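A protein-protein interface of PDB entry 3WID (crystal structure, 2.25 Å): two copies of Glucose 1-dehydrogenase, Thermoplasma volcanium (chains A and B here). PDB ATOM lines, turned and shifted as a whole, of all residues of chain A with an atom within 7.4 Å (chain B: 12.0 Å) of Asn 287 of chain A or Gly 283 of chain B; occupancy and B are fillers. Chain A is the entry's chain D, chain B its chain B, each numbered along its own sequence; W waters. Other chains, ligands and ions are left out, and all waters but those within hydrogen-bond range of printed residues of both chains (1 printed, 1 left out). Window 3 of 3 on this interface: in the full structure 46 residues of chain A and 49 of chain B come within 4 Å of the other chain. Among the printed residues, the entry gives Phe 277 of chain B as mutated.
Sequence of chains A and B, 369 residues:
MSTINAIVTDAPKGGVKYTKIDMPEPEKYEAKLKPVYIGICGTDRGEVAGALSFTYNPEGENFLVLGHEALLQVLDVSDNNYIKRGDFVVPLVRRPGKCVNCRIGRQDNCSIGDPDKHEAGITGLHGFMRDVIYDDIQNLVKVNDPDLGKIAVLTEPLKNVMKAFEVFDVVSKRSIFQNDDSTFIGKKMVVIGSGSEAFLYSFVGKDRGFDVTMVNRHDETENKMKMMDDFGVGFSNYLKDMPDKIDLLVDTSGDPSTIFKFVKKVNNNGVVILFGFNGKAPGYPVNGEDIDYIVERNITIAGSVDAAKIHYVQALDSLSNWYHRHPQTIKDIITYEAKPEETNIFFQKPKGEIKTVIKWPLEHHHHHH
The backbone carbonyl oxygen (O) of Ala 281 of chain B is in hydrogen-bond range of the backbone NH (N) of Gly 288 of chain A (3.0 Å). The backbone NH (N) of Tyr 284 of chain B lies within hydrogen-bond range of the backbone carbonyl oxygen (O) of Val 286 of chain A (3.0 Å). O of Tyr 284 of chain A lies within hydrogen-bond range of N of Val 286 of chain B (2.8 Å).
The side-chain amide oxygen of Asn 278 of chain B sits at hydrogen-bond distance from the backbone NH of Lys 280 of chain B, at 3.0 Å. ND2 of Asn 278 of chain B lies close to N of Ala 281 of chain B, 3.3 Å away. NZ of Lys 264 of chain A sits at hydrogen-bond distance from OH of Tyr 284 of chain A (3.1 Å). N of Asn 287 of chain A lies within hydrogen-bond range of OD2 of Asp 290 of chain A, at 2.6 Å.
O of Tyr 284 of chain A touches O of Tyr 284 of chain B, at 3.5 Å. O of Tyr 284 of chain A touches CA of Pro 285 of chain B, 3.4 Å away. O of Val 286 of chain A touches CA of Gly 283 of chain B, at 3.4 Å. Pro 256 of chain B touches Asn 287 of chain A (CG to C, 3.6 Å). Gly 288 of chain A touches Pro 256 of chain B. Gly 288 of chain A touches Asn 278 of chain B. CA of Gly 279 of chain B touches C of Gly 288 of chain A, 3.98 Å away.
Printed residues of chain B within 4 Å of Asn 287 of chain A: Pro 256 (3.6 Å) and Gly 283 (3.8 Å). Gly 283 of chain B touches two residues of chain A. Pro 285 of chain A touches just these residues of chain B: Tyr 284 and Pro 285. Val 286 of chain A touches just these residues of chain B: Pro 256 (3.2 Å), Phe 260 (3.8 Å), Gly 283 (3.4 Å), Tyr 284 (3.0 Å) and Val 286 (3.9 Å). Gly 288 of chain A touches four residues of chain B. No residue of chain B comes within 4 Å of Asp 290 of chain A. Printed residues of chain A within 4 Å of Gly 279 of chain B: Gly 288 (3.98 Å) and Glu 289 (3.5 Å). Of the printed residues of chain A, Tyr 284 of chain B touches Tyr 284 (3.5 Å), Pro 285 (3.5 Å) and Val 286 (3.0 Å). Tyr 293 of chain A touches none of the printed residues of chain B. The nearest printed residue of chain B that does not touch Asn 287 of chain A is Ala 281 of chain B (4.01 Å). The nearest residue of chain A that does not touch Gly 283 of chain B is Pro 285 of chain A (4.5 Å).
Printed residues of chain B that touch a printed residue of chain A: Pro 256, Phe 260, Phe 277, Asn 278, Gly 279, Ala 281, Gly 283, Tyr 284, Pro 285 and Val 286. Hydrophobic or aromatic side chains of chain B that line the printed part of chain A: Pro 256, Phe 260, Phe 277, Ala 281 and Val 286. Hydrophobic or aromatic side chains of chain A that line the printed part of chain B: Val 286.
Tyr 284 of chain A touches Pro 285 of chain B, and with the chains exchanged Pro 285 of chain A touches Tyr 284 of chain B. Tyr 284 of chain A touches Val 286 of chain B, and with the chains exchanged Val 286 of chain A touches Tyr 284 of chain B. Pro 285 of chain B touches its own counterpart, Pro 285 of chain A.
Water W1 lies within hydrogen-bond range of N of Asn 278 of chain B (2.6 Å), O of Gly 254 of chain B (2.7 Å) and O of Gly 288 of chain A (2.8 Å).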
ATOM      1  N   PHE A 260       9.976  -4.601  27.668  1.00  0.00           N
ATOM      2  CA  PHE A 260      10.323  -4.899  26.302  1.00  0.00           C
ATOM      3  C   PHE A 260      11.747  -4.541  25.967  1.00  0.00           C
ATOM      4  O   PHE A 260      12.300  -5.112  25.006  1.00  0.00           O
ATOM      5  CB  PHE A 260       9.366  -4.277  25.290  1.00  0.00           C
ATOM      6  CG  PHE A 260       8.095  -5.013  25.198  1.00  0.00           C
ATOM      7  CD1 PHE A 260       8.038  -6.225  24.502  1.00  0.00           C
ATOM      8  CD2 PHE A 260       6.984  -4.598  25.905  1.00  0.00           C
ATOM      9  CE1 PHE A 260       6.881  -6.964  24.477  1.00  0.00           C
ATOM     10  CE2 PHE A 260       5.826  -5.341  25.890  1.00  0.00           C
ATOM     11  CZ  PHE A 260       5.774  -6.527  25.175  1.00  0.00           C
ATOM     12  N   LYS A 264      14.620  -7.782  24.735  1.00  0.00           N
ATOM     13  CA  LYS A 264      15.638  -7.763  23.669  1.00  0.00           C
ATOM     14  C   LYS A 264      17.047  -8.116  24.085  1.00  0.00           C
ATOM     15  O   LYS A 264      17.935  -8.086  23.282  1.00  0.00           O
ATOM     16  CB  LYS A 264      15.672  -6.398  23.015  1.00  0.00           C
ATOM     17  CG  LYS A 264      14.357  -6.063  22.348  1.00  0.00           C
ATOM     18  CD  LYS A 264      14.585  -5.236  21.083  1.00  0.00           C
ATOM     19  CE  LYS A 264      14.587  -3.723  21.370  1.00  0.00           C
ATOM     20  NZ  LYS A 264      13.230  -3.280  21.823  1.00  0.00           N
ATOM     21  N   TYR A 284       4.462   1.333  25.562  1.00  0.00           N
ATOM     22  CA  TYR A 284       5.628   1.242  24.762  1.00  0.00           C
ATOM     23  C   TYR A 284       5.199   0.596  23.445  1.00  0.00           C
ATOM     24  O   TYR A 284       4.368  -0.328  23.413  1.00  0.00           O
ATOM     25  CB  TYR A 284       6.697   0.442  25.459  1.00  0.00           C
ATOM     26  CG  TYR A 284       7.833   0.020  24.570  1.00  0.00           C
ATOM     27  CD1 TYR A 284       7.679  -1.063  23.698  1.00  0.00           C
ATOM     28  CD2 TYR A 284       9.057   0.666  24.603  1.00  0.00           C
ATOM     29  CE1 TYR A 284       8.699  -1.478  22.874  1.00  0.00           C
ATOM     30  CE2 TYR A 284      10.096   0.251  23.786  1.00  0.00           C
ATOM     31  CZ  TYR A 284       9.903  -0.834  22.928  1.00  0.00           C
ATOM     32  OH  TYR A 284      10.879  -1.316  22.084  1.00  0.00           O
ATOM     33  N   PRO A 285       5.737   1.109  22.349  1.00  0.00           N
ATOM     34  CA  PRO A 285       5.295   0.720  21.031  1.00  0.00           C
ATOM     35  C   PRO A 285       6.063  -0.509  20.566  1.00  0.00           C
ATOM     36  O   PRO A 285       7.210  -0.402  20.137  1.00  0.00           O
ATOM     37  CB  PRO A 285       5.591   1.972  20.184  1.00  0.00           C
ATOM     38  CG  PRO A 285       6.772   2.556  20.821  1.00  0.00           C
ATOM     39  CD  PRO A 285       6.577   2.315  22.307  1.00  0.00           C
ATOM     40  N   VAL A 286       5.436  -1.680  20.705  1.00  0.00           N
ATOM     41  CA  VAL A 286       6.061  -2.939  20.291  1.00  0.00           C
ATOM     42  C   VAL A 286       5.987  -3.076  18.776  1.00  0.00           C
ATOM     43  O   VAL A 286       4.903  -3.023  18.194  1.00  0.00           O
ATOM     44  CB  VAL A 286       5.366  -4.121  20.962  1.00  0.00           C
ATOM     45  CG1 VAL A 286       5.884  -5.432  20.408  1.00  0.00           C
ATOM     46  CG2 VAL A 286       5.602  -4.065  22.468  1.00  0.00           C
ATOM     47  N   ASN A 287       7.125  -3.222  18.130  1.00  0.00           N
ATOM     48  CA  ASN A 287       7.154  -3.282  16.667  1.00  0.00           C
ATOM     49  C   ASN A 287       7.472  -4.678  16.098  1.00  0.00           C
ATOM     50  O   ASN A 287       7.770  -5.632  16.848  1.00  0.00           O
ATOM     51  CB  ASN A 287       8.167  -2.265  16.144  1.00  0.00           C
ATOM     52  CG  ASN A 287       9.593  -2.673  16.427  1.00  0.00           C
ATOM     53  OD1 ASN A 287       9.968  -3.823  16.269  1.00  0.00           O
ATOM     54  ND2 ASN A 287      10.406  -1.712  16.831  1.00  0.00           N
ATOM     55  N   GLY A 288       7.477  -4.736  14.768  1.00  0.00           N
ATOM     56  CA  GLY A 288       7.658  -5.946  13.980  1.00  0.00           C
ATOM     57  C   GLY A 288       8.906  -6.737  14.340  1.00  0.00           C
ATOM     58  O   GLY A 288       8.910  -7.974  14.321  1.00  0.00           O
ATOM     59  N   GLU A 289       9.948  -5.992  14.676  1.00  0.00           N
ATOM     60  CA  GLU A 289      11.181  -6.538  15.074  1.00  0.00           C
ATOM     61  C   GLU A 289      11.113  -7.083  16.444  1.00  0.00           C
ATOM     62  O   GLU A 289      11.730  -8.113  16.713  1.00  0.00           O
ATOM     63  CB  GLU A 289      12.277  -5.487  15.003  1.00  0.00           C
ATOM     64  CG  GLU A 289      12.496  -5.041  13.563  1.00  0.00           C
ATOM     65  CD  GLU A 289      13.866  -4.430  13.363  1.00  0.00           C
ATOM     66  OE1 GLU A 289      14.200  -3.469  14.093  1.00  0.00           O
ATOM     67  OE2 GLU A 289      14.603  -4.937  12.490  1.00  0.00           O
ATOM     68  N   ASP A 290      10.408  -6.413  17.343  1.00  0.00           N
ATOM     69  CA  ASP A 290      10.338  -6.922  18.702  1.00  0.00           C
ATOM     70  C   ASP A 290       9.753  -8.359  18.724  1.00  0.00           C
ATOM     71  O   ASP A 290      10.197  -9.210  19.506  1.00  0.00           O
ATOM     72  CB  ASP A 290       9.505  -6.041  19.590  1.00  0.00           C
ATOM     73  CG  ASP A 290      10.101  -4.646  19.764  1.00  0.00           C
ATOM     74  OD1 ASP A 290      11.283  -4.513  20.183  1.00  0.00           O
ATOM     75  OD2 ASP A 290       9.349  -3.700  19.447  1.00  0.00           O
ATOM     76  N   ILE A 291       8.770  -8.584  17.867  1.00  0.00           N
ATOM     77  CA  ILE A 291       8.053  -9.831  17.770  1.00  0.00           C
ATOM     78  C   ILE A 291       8.983 -10.857  17.132  1.00  0.00           C
ATOM     79  O   ILE A 291       9.114 -12.000  17.617  1.00  0.00           O
ATOM     80  CB  ILE A 291       6.808  -9.623  16.869  1.00  0.00           C
ATOM     81  CG1 ILE A 291       5.831  -8.653  17.538  1.00  0.00           C
ATOM     82  CG2 ILE A 291       6.115 -10.935  16.530  1.00  0.00           C
ATOM     83  CD1 ILE A 291       5.173  -9.176  18.796  1.00  0.00           C
ATOM     84  N   ASP A 292       9.592 -10.441  16.025  1.00  0.00           N
ATOM     85  CA  ASP A 292      10.546 -11.267  15.308  1.00  0.00           C
ATOM     86  C   ASP A 292      11.650 -11.779  16.256  1.00  0.00           C
ATOM     87  O   ASP A 292      12.031 -12.955  16.218  1.00  0.00           O
ATOM     88  CB  ASP A 292      11.150 -10.528  14.114  1.00  0.00           C
ATOM     89  CG  ASP A 292      12.140 -11.398  13.353  1.00  0.00           C
ATOM     90  OD1 ASP A 292      11.747 -12.450  12.803  1.00  0.00           O
ATOM     91  OD2 ASP A 292      13.329 -11.063  13.360  1.00  0.00           O
ATOM     92  N   TYR A 293      12.105 -10.897  17.146  1.00  0.00           N
ATOM     93  CA  TYR A 293      13.107 -11.244  18.143  1.00  0.00           C
ATOM     94  C   TYR A 293      12.579 -12.423  19.006  1.00  0.00           C
ATOM     95  O   TYR A 293      13.283 -13.414  19.223  1.00  0.00           O
ATOM     96  CB  TYR A 293      13.410 -10.025  18.976  1.00  0.00           C
ATOM     97  CG  TYR A 293      14.506 -10.230  19.939  1.00  0.00           C
ATOM     98  CD1 TYR A 293      14.242 -10.813  21.177  1.00  0.00           C
ATOM     99  CD2 TYR A 293      15.831  -9.821  19.638  1.00  0.00           C
ATOM    100  CE1 TYR A 293      15.254 -11.029  22.101  1.00  0.00           C
ATOM    101  CE2 TYR A 293      16.866 -10.080  20.548  1.00  0.00           C
ATOM    102  CZ  TYR A 293      16.563 -10.676  21.790  1.00  0.00           C
ATOM    103  OH  TYR A 293      17.522 -10.945  22.754  1.00  0.00           O
ATOM    104  N   ASP B 251      -0.777 -16.374  15.691  1.00  0.00           N
ATOM    105  CA  ASP B 251      -0.516 -15.352  14.709  1.00  0.00           C
ATOM    106  C   ASP B 251       0.491 -15.709  13.626  1.00  0.00           C
ATOM    107  O   ASP B 251       1.650 -16.086  13.954  1.00  0.00           O
ATOM    108  CB  ASP B 251       0.045 -14.096  15.376  1.00  0.00           C
ATOM    109  CG  ASP B 251       0.325 -13.006  14.384  1.00  0.00           C
ATOM    110  OD1 ASP B 251      -0.630 -12.601  13.624  1.00  0.00           O
ATOM    111  OD2 ASP B 251       1.523 -12.588  14.351  1.00  0.00           O
ATOM    112  N   SER B 253       0.624 -13.177  10.988  1.00  0.00           N
ATOM    113  CA  SER B 253       0.832 -11.849  10.394  1.00  0.00           C
ATOM    114  C   SER B 253       2.229 -11.260  10.706  1.00  0.00           C
ATOM    115  O   SER B 253       2.886 -10.703   9.868  1.00  0.00           O
ATOM    116  CB  SER B 253      -0.243 -10.863  10.932  1.00  0.00           C
ATOM    117  OG  SER B 253       0.064 -10.430  12.288  1.00  0.00           O
ATOM    118  N   GLY B 254       2.677 -11.370  11.937  1.00  0.00           N
ATOM    119  CA  GLY B 254       3.810 -10.638  12.363  1.00  0.00           C
ATOM    120  C   GLY B 254       3.480  -9.199  12.749  1.00  0.00           C
ATOM    121  O   GLY B 254       4.380  -8.481  13.147  1.00  0.00           O
ATOM    122  N   ASP B 255       2.194  -8.839  12.714  1.00  0.00           N
ATOM    123  CA  ASP B 255       1.706  -7.492  12.967  1.00  0.00           C
ATOM    124  C   ASP B 255       1.286  -7.210  14.444  1.00  0.00           C
ATOM    125  O   ASP B 255       0.273  -7.722  14.923  1.00  0.00           O
ATOM    126  CB  ASP B 255       0.504  -7.196  12.082  1.00  0.00           C
ATOM    127  CG  ASP B 255       0.058  -5.735  12.234  1.00  0.00           C
ATOM    128  OD1 ASP B 255       0.934  -4.882  12.189  1.00  0.00           O
ATOM    129  OD2 ASP B 255      -1.106  -5.457  12.553  1.00  0.00           O
ATOM    130  N   PRO B 256       2.054  -6.371  15.162  1.00  0.00           N
ATOM    131  CA  PRO B 256       1.864  -6.176  16.579  1.00  0.00           C
ATOM    132  C   PRO B 256       0.461  -5.732  16.987  1.00  0.00           C
ATOM    133  O   PRO B 256      -0.113  -6.209  18.009  1.00  0.00           O
ATOM    134  CB  PRO B 256       2.876  -5.097  16.889  1.00  0.00           C
ATOM    135  CG  PRO B 256       3.987  -5.400  15.988  1.00  0.00           C
ATOM    136  CD  PRO B 256       3.343  -5.863  14.717  1.00  0.00           C
ATOM    137  N   SER B 257      -0.108  -4.863  16.162  1.00  0.00           N
ATOM    138  CA  SER B 257      -1.322  -4.225  16.517  1.00  0.00           C
ATOM    139  C   SER B 257      -2.441  -5.247  16.425  1.00  0.00           C
ATOM    140  O   SER B 257      -3.315  -5.318  17.269  1.00  0.00           O
ATOM    141  CB  SER B 257      -1.543  -2.941  15.664  1.00  0.00           C
ATOM    142  OG  SER B 257      -1.793  -3.195  14.288  1.00  0.00           O
ATOM    143  N   THR B 258      -2.406  -6.075  15.415  1.00  0.00           N
ATOM    144  CA  THR B 258      -3.364  -7.191  15.303  1.00  0.00           C
ATOM    145  C   THR B 258      -3.112  -8.199  16.378  1.00  0.00           C
ATOM    146  O   THR B 258      -4.030  -8.713  16.942  1.00  0.00           O
ATOM    147  CB  THR B 258      -3.196  -7.876  13.980  1.00  0.00           C
ATOM    148  OG1 THR B 258      -3.064  -6.852  13.027  1.00  0.00           O
ATOM    149  CG2 THR B 258      -4.396  -8.720  13.635  1.00  0.00           C
ATOM    150  N   ILE B 259      -1.854  -8.443  16.686  1.00  0.00           N
ATOM    151  CA  ILE B 259      -1.526  -9.404  17.758  1.00  0.00           C
ATOM    152  C   ILE B 259      -2.075  -8.992  19.107  1.00  0.00           C
ATOM    153  O   ILE B 259      -2.836  -9.729  19.763  1.00  0.00           O
ATOM    154  CB  ILE B 259      -0.010  -9.568  17.876  1.00  0.00           C
ATOM    155  CG1 ILE B 259       0.540 -10.344  16.653  1.00  0.00           C
ATOM    156  CG2 ILE B 259       0.332 -10.324  19.118  1.00  0.00           C
ATOM    157  CD1 ILE B 259       2.035 -10.334  16.572  1.00  0.00           C
ATOM    158  N   PHE B 260      -1.664  -7.804  19.557  1.00  0.00           N
ATOM    159  CA  PHE B 260      -2.084  -7.352  20.886  1.00  0.00           C
ATOM    160  C   PHE B 260      -3.583  -7.083  21.006  1.00  0.00           C
ATOM    161  O   PHE B 260      -4.183  -7.357  22.064  1.00  0.00           O
ATOM    162  CB  PHE B 260      -1.227  -6.228  21.368  1.00  0.00           C
ATOM    163  CG  PHE B 260       0.116  -6.663  21.764  1.00  0.00           C
ATOM    164  CD1 PHE B 260       0.306  -7.341  22.957  1.00  0.00           C
ATOM    165  CD2 PHE B 260       1.195  -6.484  20.913  1.00  0.00           C
ATOM    166  CE1 PHE B 260       1.579  -7.801  23.315  1.00  0.00           C
ATOM    167  CE2 PHE B 260       2.445  -6.936  21.247  1.00  0.00           C
ATOM    168  CZ  PHE B 260       2.645  -7.572  22.462  1.00  0.00           C
ATOM    169  N   LYS B 261      -4.234  -6.659  19.917  1.00  0.00           N
ATOM    170  CA  LYS B 261      -5.684  -6.548  19.955  1.00  0.00           C
ATOM    171  C   LYS B 261      -6.384  -7.899  20.152  1.00  0.00           C
ATOM    172  O   LYS B 261      -7.420  -8.013  20.820  1.00  0.00           O
ATOM    173  CB  LYS B 261      -6.192  -5.948  18.658  1.00  0.00           C
ATOM    174  CG  LYS B 261      -5.985  -4.468  18.552  1.00  0.00           C
ATOM    175  CD  LYS B 261      -6.195  -4.006  17.139  1.00  0.00           C
ATOM    176  CE  LYS B 261      -5.910  -2.541  17.029  1.00  0.00           C
ATOM    177  NZ  LYS B 261      -6.290  -2.188  15.625  1.00  0.00           N
ATOM    178  N   LEU B 274       3.213 -16.982  18.879  1.00  0.00           N
ATOM    179  CA  LEU B 274       3.754 -16.050  17.935  1.00  0.00           C
ATOM    180  C   LEU B 274       4.539 -16.848  16.902  1.00  0.00           C
ATOM    181  O   LEU B 274       5.404 -17.607  17.256  1.00  0.00           O
ATOM    182  CB  LEU B 274       4.629 -14.997  18.625  1.00  0.00           C
ATOM    183  CG  LEU B 274       3.882 -14.051  19.557  1.00  0.00           C
ATOM    184  CD1 LEU B 274       4.804 -13.042  20.208  1.00  0.00           C
ATOM    185  CD2 LEU B 274       2.737 -13.308  18.866  1.00  0.00           C
ATOM    186  N   PHE B 275       4.215 -16.672  15.627  1.00  0.00           N
ATOM    187  CA  PHE B 275       4.819 -17.447  14.565  1.00  0.00           C
ATOM    188  C   PHE B 275       5.154 -16.598  13.341  1.00  0.00           C
ATOM    189  O   PHE B 275       6.239 -16.685  12.801  1.00  0.00           O
ATOM    190  CB  PHE B 275       3.852 -18.554  14.184  1.00  0.00           C
ATOM    191  CG  PHE B 275       4.353 -19.444  13.117  1.00  0.00           C
ATOM    192  CD1 PHE B 275       5.126 -20.506  13.447  1.00  0.00           C
ATOM    193  CD2 PHE B 275       4.018 -19.225  11.784  1.00  0.00           C
ATOM    194  CE1 PHE B 275       5.629 -21.316  12.481  1.00  0.00           C
ATOM    195  CE2 PHE B 275       4.494 -20.058  10.794  1.00  0.00           C
ATOM    196  CZ  PHE B 275       5.292 -21.129  11.159  1.00  0.00           C
ATOM    197  N   GLY B 276       4.192 -15.803  12.896  1.00  0.00           N
ATOM    198  CA  GLY B 276       4.437 -14.827  11.842  1.00  0.00           C
ATOM    199  C   GLY B 276       5.475 -13.832  12.229  1.00  0.00           C
ATOM    200  O   GLY B 276       5.553 -13.455  13.392  1.00  0.00           O
ATOM    201  N   PHE B 277       6.299 -13.395  11.285  1.00  0.00           N
ATOM    202  CA  PHE B 277       7.170 -12.257  11.581  1.00  0.00           C
ATOM    203  C   PHE B 277       7.352 -11.283  10.413  1.00  0.00           C
ATOM    204  O   PHE B 277       7.410 -11.669   9.273  1.00  0.00           O
ATOM    205  CB  PHE B 277       8.513 -12.702  12.155  1.00  0.00           C
ATOM    206  CG  PHE B 277       9.259 -13.704  11.300  1.00  0.00           C
ATOM    207  CD1 PHE B 277       9.852 -13.317  10.105  1.00  0.00           C
ATOM    208  CD2 PHE B 277       9.424 -15.029  11.724  1.00  0.00           C
ATOM    209  CE1 PHE B 277      10.537 -14.249   9.313  1.00  0.00           C
ATOM    210  CE2 PHE B 277      10.123 -15.957  10.945  1.00  0.00           C
ATOM    211  CZ  PHE B 277      10.670 -15.564   9.735  1.00  0.00           C
ATOM    212  N   ASN B 278       7.429 -10.001  10.717  1.00  0.00           N
ATOM    213  CA  ASN B 278       7.691  -8.981   9.702  1.00  0.00           C
ATOM    214  C   ASN B 278       8.341  -7.773  10.360  1.00  0.00           C
ATOM    215  O   ASN B 278       7.672  -6.993  11.051  1.00  0.00           O
ATOM    216  CB  ASN B 278       6.425  -8.600   8.971  1.00  0.00           C
ATOM    217  CG  ASN B 278       6.588  -7.327   8.180  1.00  0.00           C
ATOM    218  OD1 ASN B 278       7.623  -7.087   7.600  1.00  0.00           O
ATOM    219  ND2 ASN B 278       5.574  -6.477   8.205  1.00  0.00           N
ATOM    220  N   GLY B 279       9.651  -7.646  10.139  1.00  0.00           N
ATOM    221  CA  GLY B 279      10.430  -6.536  10.670  1.00  0.00           C
ATOM    222  C   GLY B 279       9.984  -5.140  10.244  1.00  0.00           C
ATOM    223  O   GLY B 279      10.322  -4.190  10.912  1.00  0.00           O
ATOM    224  N   LYS B 280       9.220  -5.042   9.152  1.00  0.00           N
ATOM    225  CA  LYS B 280       8.662  -3.773   8.643  1.00  0.00           C
ATOM    226  C   LYS B 280       7.306  -3.419   9.273  1.00  0.00           C
ATOM    227  O   LYS B 280       6.710  -2.412   8.912  1.00  0.00           O
ATOM    228  CB  LYS B 280       8.535  -3.824   7.097  1.00  0.00           C
ATOM    229  CG  LYS B 280       9.887  -3.899   6.380  1.00  0.00           C
ATOM    230  CD  LYS B 280       9.802  -3.984   4.851  1.00  0.00           C
ATOM    231  CE  LYS B 280       9.036  -5.204   4.339  1.00  0.00           C
ATOM    232  NZ  LYS B 280       9.641  -6.535   4.681  1.00  0.00           N
ATOM    233  N   ALA B 281       6.815  -4.214  10.221  1.00  0.00           N
ATOM    234  CA  ALA B 281       5.463  -4.005  10.711  1.00  0.00           C
ATOM    235  C   ALA B 281       5.528  -2.931  11.747  1.00  0.00           C
ATOM    236  O   ALA B 281       6.442  -2.933  12.586  1.00  0.00           O
ATOM    237  CB  ALA B 281       4.884  -5.291  11.298  1.00  0.00           C
ATOM    238  N   PRO B 282       4.570  -1.991  11.716  1.00  0.00           N
ATOM    239  CA  PRO B 282       4.717  -0.816  12.547  1.00  0.00           C
ATOM    240  C   PRO B 282       4.468  -1.082  14.006  1.00  0.00           C
ATOM    241  O   PRO B 282       3.828  -2.092  14.353  1.00  0.00           O
ATOM    242  CB  PRO B 282       3.650   0.142  12.010  1.00  0.00           C
ATOM    243  CG  PRO B 282       2.685  -0.726  11.296  1.00  0.00           C
ATOM    244  CD  PRO B 282       3.480  -1.852  10.748  1.00  0.00           C
ATOM    245  N   GLY B 283       4.950  -0.162  14.843  1.00  0.00           N
ATOM    246  CA  GLY B 283       4.835  -0.253  16.291  1.00  0.00           C
ATOM    247  C   GLY B 283       3.395  -0.093  16.745  1.00  0.00           C
ATOM    248  O   GLY B 283       2.633   0.561  16.069  1.00  0.00           O
ATOM    249  N   TYR B 284       3.015  -0.741  17.858  1.00  0.00           N
ATOM    250  CA  TYR B 284       1.684  -0.590  18.464  1.00  0.00           C
ATOM    251  C   TYR B 284       1.825  -0.488  19.967  1.00  0.00           C
ATOM    252  O   TYR B 284       2.465  -1.303  20.588  1.00  0.00           O
ATOM    253  CB  TYR B 284       0.778  -1.761  18.118  1.00  0.00           C
ATOM    254  CG  TYR B 284      -0.616  -1.630  18.646  1.00  0.00           C
ATOM    255  CD1 TYR B 284      -1.583  -0.895  17.946  1.00  0.00           C
ATOM    256  CD2 TYR B 284      -0.980  -2.213  19.869  1.00  0.00           C
ATOM    257  CE1 TYR B 284      -2.880  -0.754  18.442  1.00  0.00           C
ATOM    258  CE2 TYR B 284      -2.273  -2.094  20.361  1.00  0.00           C
ATOM    259  CZ  TYR B 284      -3.215  -1.354  19.647  1.00  0.00           C
ATOM    260  OH  TYR B 284      -4.489  -1.254  20.135  1.00  0.00           O
ATOM    261  N   PRO B 285       1.192   0.521  20.570  1.00  0.00           N
ATOM    262  CA  PRO B 285       1.434   0.755  21.965  1.00  0.00           C
ATOM    263  C   PRO B 285       0.822  -0.302  22.868  1.00  0.00           C
ATOM    264  O   PRO B 285      -0.386  -0.625  22.748  1.00  0.00           O
ATOM    265  CB  PRO B 285       0.750   2.096  22.208  1.00  0.00           C
ATOM    266  CG  PRO B 285      -0.391   2.079  21.259  1.00  0.00           C
ATOM    267  CD  PRO B 285       0.181   1.449  20.028  1.00  0.00           C
ATOM    268  N   VAL B 286       1.671  -0.781  23.785  1.00  0.00           N
ATOM    269  CA  VAL B 286       1.277  -1.711  24.808  1.00  0.00           C
ATOM    270  C   VAL B 286       1.489  -1.040  26.115  1.00  0.00           C
ATOM    271  O   VAL B 286       2.610  -0.625  26.426  1.00  0.00           O
ATOM    272  CB  VAL B 286       2.139  -3.005  24.774  1.00  0.00           C
ATOM    273  CG1 VAL B 286       1.815  -3.887  25.951  1.00  0.00           C
ATOM    274  CG2 VAL B 286       1.874  -3.777  23.499  1.00  0.00           C
ATOM    275  N   ASN B 287       0.445  -1.048  26.930  1.00  0.00           N
ATOM    276  CA  ASN B 287       0.459  -0.324  28.204  1.00  0.00           C
ATOM    277  C   ASN B 287       0.353  -1.203  29.470  1.00  0.00           C
ATOM    278  O   ASN B 287       0.228  -2.443  29.395  1.00  0.00           O
ATOM    279  CB  ASN B 287      -0.631   0.769  28.207  1.00  0.00           C
ATOM    280  CG  ASN B 287      -2.008   0.208  28.164  1.00  0.00           C
ATOM    281  OD1 ASN B 287      -2.324  -0.721  28.901  1.00  0.00           O
ATOM    282  ND2 ASN B 287      -2.857   0.773  27.306  1.00  0.00           N
ATOM    283  N   ASP B 290      -2.359  -3.650  29.645  1.00  0.00           N
ATOM    284  CA  ASP B 290      -2.237  -4.774  28.719  1.00  0.00           C
ATOM    285  C   ASP B 290      -1.424  -5.893  29.369  1.00  0.00           C
ATOM    286  O   ASP B 290      -1.859  -7.047  29.372  1.00  0.00           O
ATOM    287  CB  ASP B 290      -1.614  -4.325  27.408  1.00  0.00           C
ATOM    288  CG  ASP B 290      -2.541  -3.378  26.604  1.00  0.00           C
ATOM    289  OD1 ASP B 290      -3.767  -3.476  26.777  1.00  0.00           O
ATOM    290  OD2 ASP B 290      -2.029  -2.541  25.824  1.00  0.00           O
ATOM    291  N   ILE B 301       2.633 -16.508  26.225  1.00  0.00           N
ATOM    292  CA  ILE B 301       2.850 -16.036  24.856  1.00  0.00           C
ATOM    293  C   ILE B 301       4.160 -16.643  24.448  1.00  0.00           C
ATOM    294  O   ILE B 301       5.212 -16.240  24.965  1.00  0.00           O
ATOM    295  CB  ILE B 301       3.002 -14.504  24.806  1.00  0.00           C
ATOM    296  CG1 ILE B 301       1.705 -13.866  25.265  1.00  0.00           C
ATOM    297  CG2 ILE B 301       3.391 -14.023  23.418  1.00  0.00           C
ATOM    298  CD1 ILE B 301       1.793 -12.374  25.521  1.00  0.00           C
HETATM  299  O   HOH W   1       6.863  -9.514  13.178  1.00  0.00           O
